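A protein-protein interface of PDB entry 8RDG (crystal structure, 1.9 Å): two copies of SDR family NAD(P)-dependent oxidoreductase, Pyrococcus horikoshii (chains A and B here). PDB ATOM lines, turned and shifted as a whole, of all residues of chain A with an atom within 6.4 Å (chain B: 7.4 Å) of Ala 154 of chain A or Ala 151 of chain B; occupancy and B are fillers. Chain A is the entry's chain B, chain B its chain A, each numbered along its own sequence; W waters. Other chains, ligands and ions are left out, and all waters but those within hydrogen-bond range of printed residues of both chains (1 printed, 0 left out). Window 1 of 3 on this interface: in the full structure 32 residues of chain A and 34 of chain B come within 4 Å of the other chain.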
ATOM      1  N   VAL A  97     -10.048  31.718   5.420  1.00  0.00           N
ATOM      2  CA  VAL A  97     -10.759  30.486   5.107  1.00  0.00           C
ATOM      3  C   VAL A  97     -11.415  30.576   3.742  1.00  0.00           C
ATOM      4  O   VAL A  97     -11.263  29.675   2.908  1.00  0.00           O
ATOM      5  CB  VAL A  97     -11.795  30.165   6.196  1.00  0.00           C
ATOM      6  CG1 VAL A  97     -12.472  28.820   5.888  1.00  0.00           C
ATOM      7  CG2 VAL A  97     -11.128  30.160   7.570  1.00  0.00           C
ATOM      8  N   ALA A 147      -6.602  30.917  14.439  1.00  0.00           N
ATOM      9  CA  ALA A 147      -7.603  29.897  14.131  1.00  0.00           C
ATOM     10  C   ALA A 147      -7.917  29.857  12.639  1.00  0.00           C
ATOM     11  O   ALA A 147      -8.075  28.778  12.059  1.00  0.00           O
ATOM     12  CB  ALA A 147      -8.879  30.149  14.938  1.00  0.00           C
ATOM     13  N   LYS A 149      -5.936  30.716  10.161  1.00  0.00           N
ATOM     14  CA  LYS A 149      -4.805  30.079   9.483  1.00  0.00           C
ATOM     15  C   LYS A 149      -4.849  28.567   9.636  1.00  0.00           C
ATOM     16  O   LYS A 149      -4.641  27.829   8.660  1.00  0.00           O
ATOM     17  CB  LYS A 149      -3.458  30.615   9.996  1.00  0.00           C
ATOM     18  CG  LYS A 149      -3.063  31.957   9.405  1.00  0.00           C
ATOM     19  CD  LYS A 149      -2.846  31.820   7.898  1.00  0.00           C
ATOM     20  CE  LYS A 149      -2.233  33.070   7.298  1.00  0.00           C
ATOM     21  NZ  LYS A 149      -1.906  32.889   5.840  1.00  0.00           N
ATOM     22  N   LEU A 150      -5.136  28.083  10.850  1.00  0.00           N
ATOM     23  CA  LEU A 150      -5.216  26.638  11.050  1.00  0.00           C
ATOM     24  C   LEU A 150      -6.351  26.027  10.225  1.00  0.00           C
ATOM     25  O   LEU A 150      -6.205  24.937   9.655  1.00  0.00           O
ATOM     26  CB  LEU A 150      -5.398  26.330  12.534  1.00  0.00           C
ATOM     27  CG  LEU A 150      -5.367  24.844  12.879  1.00  0.00           C
ATOM     28  CD1 LEU A 150      -4.093  24.233  12.310  1.00  0.00           C
ATOM     29  CD2 LEU A 150      -5.442  24.637  14.380  1.00  0.00           C
ATOM     30  N   ALA A 151      -7.489  26.721  10.141  1.00  0.00           N
ATOM     31  CA  ALA A 151      -8.589  26.242   9.308  1.00  0.00           C
ATOM     32  C   ALA A 151      -8.163  26.114   7.854  1.00  0.00           C
ATOM     33  O   ALA A 151      -8.475  25.112   7.189  1.00  0.00           O
ATOM     34  CB  ALA A 151      -9.774  27.190   9.420  1.00  0.00           C
ATOM     35  N   ALA A 152      -7.429  27.115   7.350  1.00  0.00           N
ATOM     36  CA  ALA A 152      -6.912  27.033   5.986  1.00  0.00           C
ATOM     37  C   ALA A 152      -5.992  25.836   5.801  1.00  0.00           C
ATOM     38  O   ALA A 152      -6.079  25.139   4.777  1.00  0.00           O
ATOM     39  CB  ALA A 152      -6.175  28.322   5.612  1.00  0.00           C
ATOM     40  N   GLU A 153      -5.086  25.590   6.760  1.00  0.00           N
ATOM     41  CA  GLU A 153      -4.217  24.405   6.662  1.00  0.00           C
ATOM     42  C   GLU A 153      -5.040  23.133   6.537  1.00  0.00           C
ATOM     43  O   GLU A 153      -4.738  22.249   5.716  1.00  0.00           O
ATOM     44  CB  GLU A 153      -3.308  24.246   7.889  1.00  0.00           C
ATOM     45  CG  GLU A 153      -2.266  25.303   8.175  1.00  0.00           C
ATOM     46  CD  GLU A 153      -1.317  24.858   9.299  1.00  0.00           C
ATOM     47  OE1 GLU A 153      -1.449  23.707   9.775  1.00  0.00           O
ATOM     48  OE2 GLU A 153      -0.454  25.657   9.718  1.00  0.00           O
ATOM     49  N   ALA A 154      -6.051  22.993   7.399  1.00  0.00           N
ATOM     50  CA  ALA A 154      -6.854  21.776   7.389  1.00  0.00           C
ATOM     51  C   ALA A 154      -7.504  21.566   6.025  1.00  0.00           C
ATOM     52  O   ALA A 154      -7.425  20.472   5.440  1.00  0.00           O
ATOM     53  CB  ALA A 154      -7.908  21.845   8.495  1.00  0.00           C
ATOM     54  N   LEU A 155      -8.151  22.614   5.497  1.00  0.00           N
ATOM     55  CA  LEU A 155      -8.801  22.482   4.197  1.00  0.00           C
ATOM     56  C   LEU A 155      -7.810  22.081   3.119  1.00  0.00           C
ATOM     57  O   LEU A 155      -8.115  21.230   2.267  1.00  0.00           O
ATOM     58  CB  LEU A 155      -9.485  23.793   3.810  1.00  0.00           C
ATOM     59  CG  LEU A 155     -10.711  24.091   4.666  1.00  0.00           C
ATOM     60  CD1 LEU A 155     -11.335  25.427   4.266  1.00  0.00           C
ATOM     61  CD2 LEU A 155     -11.706  22.947   4.539  1.00  0.00           C
ATOM     62  N   ILE A 156      -6.626  22.707   3.128  1.00  0.00           N
ATOM     63  CA  ILE A 156      -5.597  22.377   2.148  1.00  0.00           C
ATOM     64  C   ILE A 156      -5.247  20.897   2.222  1.00  0.00           C
ATOM     65  O   ILE A 156      -5.207  20.198   1.210  1.00  0.00           O
ATOM     66  CB  ILE A 156      -4.357  23.261   2.366  1.00  0.00           C
ATOM     67  CG1 ILE A 156      -4.665  24.696   1.901  1.00  0.00           C
ATOM     68  CG2 ILE A 156      -3.152  22.706   1.592  1.00  0.00           C
ATOM     69  CD1 ILE A 156      -3.670  25.757   2.398  1.00  0.00           C
ATOM     70  N   SER A 157      -5.014  20.393   3.432  1.00  0.00           N
ATOM     71  CA  SER A 157      -4.609  18.996   3.578  1.00  0.00           C
ATOM     72  C   SER A 157      -5.683  18.053   3.033  1.00  0.00           C
ATOM     73  O   SER A 157      -5.389  17.123   2.258  1.00  0.00           O
ATOM     74  CB  SER A 157      -4.308  18.712   5.053  1.00  0.00           C
ATOM     75  OG  SER A 157      -4.148  17.323   5.290  1.00  0.00           O
ATOM     76  N   GLY A 158      -6.947  18.302   3.403  1.00  0.00           N
ATOM     77  CA  GLY A 158      -8.027  17.429   2.948  1.00  0.00           C
ATOM     78  C   GLY A 158      -8.226  17.458   1.442  1.00  0.00           C
ATOM     79  O   GLY A 158      -8.430  16.410   0.808  1.00  0.00           O
ATOM     80  N   TYR A 159      -8.169  18.653   0.843  1.00  0.00           N
ATOM     81  CA  TYR A 159      -8.290  18.744  -0.610  1.00  0.00           C
ATOM     82  C   TYR A 159      -7.114  18.084  -1.294  1.00  0.00           C
ATOM     83  O   TYR A 159      -7.273  17.456  -2.348  1.00  0.00           O
ATOM     84  CB  TYR A 159      -8.382  20.197  -1.057  1.00  0.00           C
ATOM     85  CG  TYR A 159      -9.781  20.750  -1.069  1.00  0.00           C
ATOM     86  CD1 TYR A 159     -10.476  21.003   0.109  1.00  0.00           C
ATOM     87  CD2 TYR A 159     -10.402  21.041  -2.276  1.00  0.00           C
ATOM     88  CE1 TYR A 159     -11.781  21.528   0.077  1.00  0.00           C
ATOM     89  CE2 TYR A 159     -11.676  21.567  -2.319  1.00  0.00           C
ATOM     90  CZ  TYR A 159     -12.361  21.803  -1.158  1.00  0.00           C
ATOM     91  OH  TYR A 159     -13.627  22.324  -1.292  1.00  0.00           O
ATOM     92  N   ILE A 169       3.069  23.121   3.568  1.00  0.00           N
ATOM     93  CA  ILE A 169       2.551  24.098   4.513  1.00  0.00           C
ATOM     94  C   ILE A 169       3.725  24.607   5.333  1.00  0.00           C
ATOM     95  O   ILE A 169       4.385  23.827   6.027  1.00  0.00           O
ATOM     96  CB  ILE A 169       1.458  23.475   5.395  1.00  0.00           C
ATOM     97  CG1 ILE A 169       0.258  23.112   4.511  1.00  0.00           C
ATOM     98  CG2 ILE A 169       1.048  24.451   6.500  1.00  0.00           C
ATOM     99  CD1 ILE A 169      -0.728  22.201   5.166  1.00  0.00           C
ATOM    100  N   TYR B  93     -18.119  21.583   3.184  1.00  0.00           N
ATOM    101  CA  TYR B  93     -17.625  22.867   3.680  1.00  0.00           C
ATOM    102  C   TYR B  93     -18.747  23.677   4.324  1.00  0.00           C
ATOM    103  O   TYR B  93     -18.584  24.219   5.422  1.00  0.00           O
ATOM    104  CB  TYR B  93     -16.957  23.663   2.546  1.00  0.00           C
ATOM    105  CG  TYR B  93     -16.776  25.129   2.896  1.00  0.00           C
ATOM    106  CD1 TYR B  93     -15.666  25.591   3.602  1.00  0.00           C
ATOM    107  CD2 TYR B  93     -17.747  26.046   2.547  1.00  0.00           C
ATOM    108  CE1 TYR B  93     -15.546  26.946   3.937  1.00  0.00           C
ATOM    109  CE2 TYR B  93     -17.632  27.381   2.870  1.00  0.00           C
ATOM    110  CZ  TYR B  93     -16.548  27.826   3.558  1.00  0.00           C
ATOM    111  OH  TYR B  93     -16.487  29.171   3.850  1.00  0.00           O
ATOM    112  N   ASN B  96     -20.115  22.028   7.640  1.00  0.00           N
ATOM    113  CA  ASN B  96     -19.176  21.862   8.739  1.00  0.00           C
ATOM    114  C   ASN B  96     -18.410  23.131   9.065  1.00  0.00           C
ATOM    115  O   ASN B  96     -18.333  23.501  10.243  1.00  0.00           O
ATOM    116  CB  ASN B  96     -18.217  20.706   8.439  1.00  0.00           C
ATOM    117  CG  ASN B  96     -18.918  19.368   8.479  1.00  0.00           C
ATOM    118  OD1 ASN B  96     -19.031  18.757   9.538  1.00  0.00           O
ATOM    119  ND2 ASN B  96     -19.422  18.918   7.333  1.00  0.00           N
ATOM    120  N   VAL B  97     -17.828  23.813   8.072  1.00  0.00           N
ATOM    121  CA  VAL B  97     -17.069  25.023   8.378  1.00  0.00           C
ATOM    122  C   VAL B  97     -17.990  26.233   8.484  1.00  0.00           C
ATOM    123  O   VAL B  97     -17.982  26.939   9.496  1.00  0.00           O
ATOM    124  CB  VAL B  97     -15.957  25.272   7.335  1.00  0.00           C
ATOM    125  CG1 VAL B  97     -15.102  26.464   7.765  1.00  0.00           C
ATOM    126  CG2 VAL B  97     -15.095  24.017   7.142  1.00  0.00           C
ATOM    127  N   THR B 100     -20.561  26.399  11.403  1.00  0.00           N
ATOM    128  CA  THR B 100     -19.873  26.556  12.688  1.00  0.00           C
ATOM    129  C   THR B 100     -19.388  27.980  12.854  1.00  0.00           C
ATOM    130  O   THR B 100     -19.492  28.557  13.943  1.00  0.00           O
ATOM    131  CB  THR B 100     -18.699  25.585  12.811  1.00  0.00           C
ATOM    132  OG1 THR B 100     -19.175  24.241  12.737  1.00  0.00           O
ATOM    133  CG2 THR B 100     -17.936  25.797  14.142  1.00  0.00           C
ATOM    134  N   LEU B 104     -20.434  30.531  15.788  1.00  0.00           N
ATOM    135  CA  LEU B 104     -19.455  31.210  16.621  1.00  0.00           C
ATOM    136  C   LEU B 104     -19.684  32.720  16.617  1.00  0.00           C
ATOM    137  O   LEU B 104     -19.527  33.378  17.654  1.00  0.00           O
ATOM    138  CB  LEU B 104     -18.042  30.850  16.158  1.00  0.00           C
ATOM    139  CG  LEU B 104     -17.599  29.409  16.443  1.00  0.00           C
ATOM    140  CD1 LEU B 104     -16.348  29.036  15.636  1.00  0.00           C
ATOM    141  CD2 LEU B 104     -17.361  29.199  17.935  1.00  0.00           C
ATOM    142  N   PHE B 117     -18.650  20.432  21.118  1.00  0.00           N
ATOM    143  CA  PHE B 117     -18.597  20.160  19.688  1.00  0.00           C
ATOM    144  C   PHE B 117     -18.278  18.692  19.459  1.00  0.00           C
ATOM    145  O   PHE B 117     -17.291  18.175  20.000  1.00  0.00           O
ATOM    146  CB  PHE B 117     -17.550  21.050  19.007  1.00  0.00           C
ATOM    147  CG  PHE B 117     -17.410  20.815  17.519  1.00  0.00           C
ATOM    148  CD1 PHE B 117     -18.508  20.878  16.675  1.00  0.00           C
ATOM    149  CD2 PHE B 117     -16.159  20.575  16.964  1.00  0.00           C
ATOM    150  CE1 PHE B 117     -18.364  20.672  15.305  1.00  0.00           C
ATOM    151  CE2 PHE B 117     -16.009  20.392  15.596  1.00  0.00           C
ATOM    152  CZ  PHE B 117     -17.112  20.435  14.766  1.00  0.00           C
ATOM    153  N   VAL B 123     -10.258  13.933  11.876  1.00  0.00           N
ATOM    154  CA  VAL B 123      -9.293  15.025  11.934  1.00  0.00           C
ATOM    155  C   VAL B 123      -7.871  14.488  11.997  1.00  0.00           C
ATOM    156  O   VAL B 123      -6.934  15.192  11.607  1.00  0.00           O
ATOM    157  CB  VAL B 123      -9.537  15.969  13.137  1.00  0.00           C
ATOM    158  CG1 VAL B 123     -10.958  16.528  13.117  1.00  0.00           C
ATOM    159  CG2 VAL B 123      -9.227  15.273  14.463  1.00  0.00           C
ATOM    160  N   LEU B 139      -1.649  17.172  12.544  1.00  0.00           N
ATOM    161  CA  LEU B 139      -2.975  16.747  12.117  1.00  0.00           C
ATOM    162  C   LEU B 139      -3.065  16.933  10.611  1.00  0.00           C
ATOM    163  O   LEU B 139      -2.895  18.051  10.111  1.00  0.00           O
ATOM    164  CB  LEU B 139      -4.069  17.534  12.843  1.00  0.00           C
ATOM    165  CG  LEU B 139      -4.216  17.198  14.327  1.00  0.00           C
ATOM    166  CD1 LEU B 139      -5.435  17.865  14.953  1.00  0.00           C
ATOM    167  CD2 LEU B 139      -4.333  15.706  14.500  1.00  0.00           C
ATOM    168  N   GLU B 140      -3.324  15.843   9.894  1.00  0.00           N
ATOM    169  CA  GLU B 140      -3.270  15.817   8.427  1.00  0.00           C
ATOM    170  C   GLU B 140      -4.481  15.050   7.903  1.00  0.00           C
ATOM    171  O   GLU B 140      -4.371  13.906   7.453  1.00  0.00           O
ATOM    172  CB  GLU B 140      -1.957  15.177   7.950  1.00  0.00           C
ATOM    173  CG  GLU B 140      -1.771  15.128   6.423  1.00  0.00           C
ATOM    174  CD  GLU B 140      -0.567  14.274   5.977  1.00  0.00           C
ATOM    175  OE1 GLU B 140       0.354  14.030   6.789  1.00  0.00           O
ATOM    176  OE2 GLU B 140      -0.569  13.825   4.805  1.00  0.00           O
ATOM    177  N   PRO B 141      -5.669  15.650   7.966  1.00  0.00           N
ATOM    178  CA  PRO B 141      -6.860  14.943   7.484  1.00  0.00           C
ATOM    179  C   PRO B 141      -6.752  14.636   6.000  1.00  0.00           C
ATOM    180  O   PRO B 141      -6.174  15.400   5.225  1.00  0.00           O
ATOM    181  CB  PRO B 141      -8.004  15.926   7.772  1.00  0.00           C
ATOM    182  CG  PRO B 141      -7.346  17.266   7.989  1.00  0.00           C
ATOM    183  CD  PRO B 141      -5.974  16.989   8.505  1.00  0.00           C
ATOM    184  N   ILE B 142      -7.322  13.503   5.607  1.00  0.00           N
ATOM    185  CA  ILE B 142      -7.241  13.034   4.228  1.00  0.00           C
ATOM    186  C   ILE B 142      -8.563  13.148   3.503  1.00  0.00           C
ATOM    187  O   ILE B 142      -8.637  12.788   2.327  1.00  0.00           O
ATOM    188  CB  ILE B 142      -6.723  11.584   4.140  1.00  0.00           C
ATOM    189  CG1 ILE B 142      -7.741  10.593   4.730  1.00  0.00           C
ATOM    190  CG2 ILE B 142      -5.388  11.451   4.835  1.00  0.00           C
ATOM    191  CD1 ILE B 142      -7.345   9.125   4.463  1.00  0.00           C
ATOM    192  N   SER B 143      -9.614  13.625   4.163  1.00  0.00           N
ATOM    193  CA  SER B 143     -10.884  13.817   3.495  1.00  0.00           C
ATOM    194  C   SER B 143     -11.323  15.264   3.653  1.00  0.00           C
ATOM    195  O   SER B 143     -10.912  15.972   4.583  1.00  0.00           O
ATOM    196  CB  SER B 143     -11.963  12.884   4.055  1.00  0.00           C
ATOM    197  OG  SER B 143     -12.184  13.129   5.447  1.00  0.00           O
ATOM    198  N   VAL B 144     -12.189  15.692   2.737  1.00  0.00           N
ATOM    199  CA  VAL B 144     -12.782  17.016   2.888  1.00  0.00           C
ATOM    200  C   VAL B 144     -13.580  17.089   4.180  1.00  0.00           C
ATOM    201  O   VAL B 144     -13.597  18.130   4.845  1.00  0.00           O
ATOM    202  CB  VAL B 144     -13.651  17.361   1.661  1.00  0.00           C
ATOM    203  CG1 VAL B 144     -14.447  18.641   1.913  1.00  0.00           C
ATOM    204  CG2 VAL B 144     -12.755  17.542   0.427  1.00  0.00           C
ATOM    205  N   TYR B 145     -14.225  15.988   4.575  1.00  0.00           N
ATOM    206  CA  TYR B 145     -15.003  15.995   5.813  1.00  0.00           C
ATOM    207  C   TYR B 145     -14.104  16.171   7.033  1.00  0.00           C
ATOM    208  O   TYR B 145     -14.385  17.002   7.911  1.00  0.00           O
ATOM    209  CB  TYR B 145     -15.808  14.704   5.927  1.00  0.00           C
ATOM    210  CG  TYR B 145     -16.441  14.484   7.294  1.00  0.00           C
ATOM    211  CD1 TYR B 145     -17.594  15.174   7.665  1.00  0.00           C
ATOM    212  CD2 TYR B 145     -15.909  13.565   8.195  1.00  0.00           C
ATOM    213  CE1 TYR B 145     -18.184  14.971   8.893  1.00  0.00           C
ATOM    214  CE2 TYR B 145     -16.499  13.345   9.424  1.00  0.00           C
ATOM    215  CZ  TYR B 145     -17.647  14.053   9.771  1.00  0.00           C
ATOM    216  OH  TYR B 145     -18.247  13.853  10.999  1.00  0.00           O
ATOM    217  N   GLY B 146     -13.026  15.383   7.111  1.00  0.00           N
ATOM    218  CA  GLY B 146     -12.118  15.498   8.238  1.00  0.00           C
ATOM    219  C   GLY B 146     -11.428  16.844   8.277  1.00  0.00           C
ATOM    220  O   GLY B 146     -11.223  17.419   9.351  1.00  0.00           O
ATOM    221  N   ALA B 147     -11.072  17.373   7.101  1.00  0.00           N
ATOM    222  CA  ALA B 147     -10.530  18.727   7.040  1.00  0.00           C
ATOM    223  C   ALA B 147     -11.531  19.750   7.554  1.00  0.00           C
ATOM    224  O   ALA B 147     -11.159  20.683   8.273  1.00  0.00           O
ATOM    225  CB  ALA B 147     -10.147  19.079   5.602  1.00  0.00           C
ATOM    226  N   ALA B 148     -12.810  19.604   7.183  1.00  0.00           N
ATOM    227  CA  ALA B 148     -13.812  20.579   7.605  1.00  0.00           C
ATOM    228  C   ALA B 148     -14.038  20.507   9.108  1.00  0.00           C
ATOM    229  O   ALA B 148     -14.178  21.542   9.772  1.00  0.00           O
ATOM    230  CB  ALA B 148     -15.118  20.360   6.838  1.00  0.00           C
ATOM    231  N   LYS B 149     -14.027  19.293   9.663  1.00  0.00           N
ATOM    232  CA  LYS B 149     -14.124  19.131  11.112  1.00  0.00           C
ATOM    233  C   LYS B 149     -12.939  19.770  11.820  1.00  0.00           C
ATOM    234  O   LYS B 149     -13.105  20.422  12.859  1.00  0.00           O
ATOM    235  CB  LYS B 149     -14.211  17.648  11.458  1.00  0.00           C
ATOM    236  CG  LYS B 149     -15.578  17.068  11.216  1.00  0.00           C
ATOM    237  CD  LYS B 149     -16.551  17.744  12.154  1.00  0.00           C
ATOM    238  CE  LYS B 149     -17.867  17.029  12.196  1.00  0.00           C
ATOM    239  NZ  LYS B 149     -18.794  17.631  13.215  1.00  0.00           N
ATOM    240  N   LEU B 150     -11.721  19.577  11.286  1.00  0.00           N
ATOM    241  CA  LEU B 150     -10.545  20.195  11.905  1.00  0.00           C
ATOM    242  C   LEU B 150     -10.610  21.725  11.823  1.00  0.00           C
ATOM    243  O   LEU B 150     -10.267  22.434  12.787  1.00  0.00           O
ATOM    244  CB  LEU B 150      -9.270  19.660  11.238  1.00  0.00           C
ATOM    245  CG  LEU B 150      -7.942  20.108  11.863  1.00  0.00           C
ATOM    246  CD1 LEU B 150      -7.931  19.821  13.346  1.00  0.00           C
ATOM    247  CD2 LEU B 150      -6.770  19.395  11.190  1.00  0.00           C
ATOM    248  N   ALA B 151     -11.070  22.252  10.683  1.00  0.00           N
ATOM    249  CA  ALA B 151     -11.234  23.694  10.535  1.00  0.00           C
ATOM    250  C   ALA B 151     -12.240  24.241  11.546  1.00  0.00           C
ATOM    251  O   ALA B 151     -12.047  25.324  12.127  1.00  0.00           O
ATOM    252  CB  ALA B 151     -11.665  24.017   9.095  1.00  0.00           C
ATOM    253  N   ALA B 152     -13.328  23.508  11.756  1.00  0.00           N
ATOM    254  CA  ALA B 152     -14.313  23.901  12.757  1.00  0.00           C
ATOM    255  C   ALA B 152     -13.707  23.922  14.162  1.00  0.00           C
ATOM    256  O   ALA B 152     -13.942  24.862  14.931  1.00  0.00           O
ATOM    257  CB  ALA B 152     -15.516  22.956  12.668  1.00  0.00           C
ATOM    258  N   GLU B 153     -12.928  22.890  14.517  1.00  0.00           N
ATOM    259  CA  GLU B 153     -12.250  22.889  15.819  1.00  0.00           C
ATOM    260  C   GLU B 153     -11.390  24.132  15.990  1.00  0.00           C
ATOM    261  O   GLU B 153     -11.366  24.758  17.062  1.00  0.00           O
ATOM    262  CB  GLU B 153     -11.344  21.664  15.978  1.00  0.00           C
ATOM    263  CG  GLU B 153     -11.975  20.287  16.042  1.00  0.00           C
ATOM    264  CD  GLU B 153     -10.920  19.204  16.419  1.00  0.00           C
ATOM    265  OE1 GLU B 153      -9.733  19.568  16.625  1.00  0.00           O
ATOM    266  OE2 GLU B 153     -11.274  18.005  16.553  1.00  0.00           O
ATOM    267  N   ALA B 154     -10.596  24.445  14.965  1.00  0.00           N
ATOM    268  CA  ALA B 154      -9.716  25.603  15.044  1.00  0.00           C
ATOM    269  C   ALA B 154     -10.507  26.887  15.291  1.00  0.00           C
ATOM    270  O   ALA B 154     -10.155  27.692  16.173  1.00  0.00           O
ATOM    271  CB  ALA B 154      -8.888  25.695  13.762  1.00  0.00           C
ATOM    272  N   LEU B 155     -11.570  27.115  14.503  1.00  0.00           N
ATOM    273  CA  LEU B 155     -12.363  28.330  14.709  1.00  0.00           C
ATOM    274  C   LEU B 155     -12.936  28.370  16.121  1.00  0.00           C
ATOM    275  O   LEU B 155     -12.951  29.425  16.766  1.00  0.00           O
ATOM    276  CB  LEU B 155     -13.489  28.427  13.680  1.00  0.00           C
ATOM    277  CG  LEU B 155     -13.047  28.653  12.229  1.00  0.00           C
ATOM    278  CD1 LEU B 155     -14.264  28.635  11.341  1.00  0.00           C
ATOM    279  CD2 LEU B 155     -12.265  29.962  12.044  1.00  0.00           C
ATOM    280  N   ILE B 156     -13.420  27.225  16.610  1.00  0.00           N
ATOM    281  CA  ILE B 156     -13.962  27.164  17.966  1.00  0.00           C
ATOM    282  C   ILE B 156     -12.915  27.597  18.985  1.00  0.00           C
ATOM    283  O   ILE B 156     -13.199  28.371  19.903  1.00  0.00           O
ATOM    284  CB  ILE B 156     -14.482  25.748  18.261  1.00  0.00           C
ATOM    285  CG1 ILE B 156     -15.775  25.495  17.472  1.00  0.00           C
ATOM    286  CG2 ILE B 156     -14.733  25.600  19.750  1.00  0.00           C
ATOM    287  CD1 ILE B 156     -16.138  24.028  17.354  1.00  0.00           C
ATOM    288  N   SER B 157     -11.696  27.082  18.856  1.00  0.00           N
ATOM    289  CA  SER B 157     -10.653  27.423  19.822  1.00  0.00           C
ATOM    290  C   SER B 157     -10.356  28.923  19.796  1.00  0.00           C
ATOM    291  O   SER B 157     -10.292  29.585  20.846  1.00  0.00           O
ATOM    292  CB  SER B 157      -9.396  26.605  19.534  1.00  0.00           C
ATOM    293  OG  SER B 157      -8.321  27.061  20.330  1.00  0.00           O
HETATM  294  O   HOH W   1      -2.969  21.342  10.697  1.00  0.00           O
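O of Pro 141 of chain B lies within hydrogen-bond range of OG of Ser 157 of chain A (2.8 Å).
OG of Ser 143 of chain B sits at hydrogen-bond distance from N of Gly 146 of chain B, 2.9 Å away.
Among the printed residues, pairs that only touch across the chains: Val 97 of chain A with Val 97 of chain B (3.999 Å), Ala 147 of chain A with Ala 154 of chain B (3.0 Å), Ala 147 of chain A with Leu 155 of chain B (3.9 Å), Leu 150 of chain A with Ala 154 of chain B (3.7 Å), Ala 151 of chain A with Ala 151 of chain B (3.7 Å), Ala 154 of chain A with Ala 147 of chain B (3.1 Å), Ala 154 of chain A with Leu 150 of chain B (3.8 Å), Ala 154 of chain A with Ala 151 of chain B (3.9 Å), Leu 155 of chain A with Ala 147 of chain B (3.9 Å), Ser 157 of chain A with Glu 140 of chain B (3.4 Å), Gly 158 of chain A with Pro 141 of chain B (3.5 Å), Gly 158 of chain A with Ile 142 of chain B (3.9 Å), Gly 158 of chain A with Ser 143 of chain B (3.6 Å) and Gly 158 of chain A with Ala 147 of chain B (3.8 Å).
Ala 154 of chain A touches three residues of chain B.
Of the printed residues of chain A, Val 97 of chain B touches Val 97 (3.999 Å).
Of the printed residues of chain B, Ser 157 of chain A touches Glu 140 (3.4 Å) and Pro 141 (2.8 Å).
Printed residues of chain B within 4 Å of Ala 147 of chain A: Ala 154 and Leu 155.
Of the printed residues of chain A, Ala 154 of chain B touches Ala 147 and Leu 150.
Tyr 145 of chain B touches none of the printed residues of chain A.
The nearest residue of chain B that does not touch Ala 154 of chain A is Pro 141 of chain B (4.1 Å).
The nearest printed residue of chain B that does not touch Val 97 of chain A is Tyr 93 of chain B (4.1 Å).
Of the 26 printed residues of chain B, 10 touch a printed residue of chain A.
Hydrophobic or aromatic side chains of chain B that line the printed part of chain A: Val 97, Pro 141, Ala 147, Leu 150, Ala 151 and Ala 154.
Along chain B the printed residues that touch a printed residue of chain A span positions 97 to 155.
Hydrophobic or aromatic side chains of chain A within 4 Å of the printed part of chain B: Val 97, Ala 147, Leu 150, Ala 151 and Ala 154.
Along chain A the printed residues that touch a printed residue of chain B span positions 97 to 158.
Among the printed residues, 15 pairs touch across the chains.
Among the printed residues, no Asp or Glu carboxylate lies within 4 Å of a Lys or Arg side-chain nitrogen of the other chain.
Val 97 of chain A touches its own counterpart, Val 97 of chain B.
Leu 150 of chain A touches Ala 154 of chain B, and with the chains exchanged Ala 154 of chain A touches Leu 150 of chain B.
Ala 151 of chain A touches its own counterpart, Ala 151 of chain B.
Ala 154 of chain A touches Ala 151 of chain B, but with the chains exchanged Ala 151 of chain A does not touch Ala 154 of chain B (4.02 Å).
Water W1 bridges OE1 of Glu 153 of chain A and O of Leu 139 of chain B.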
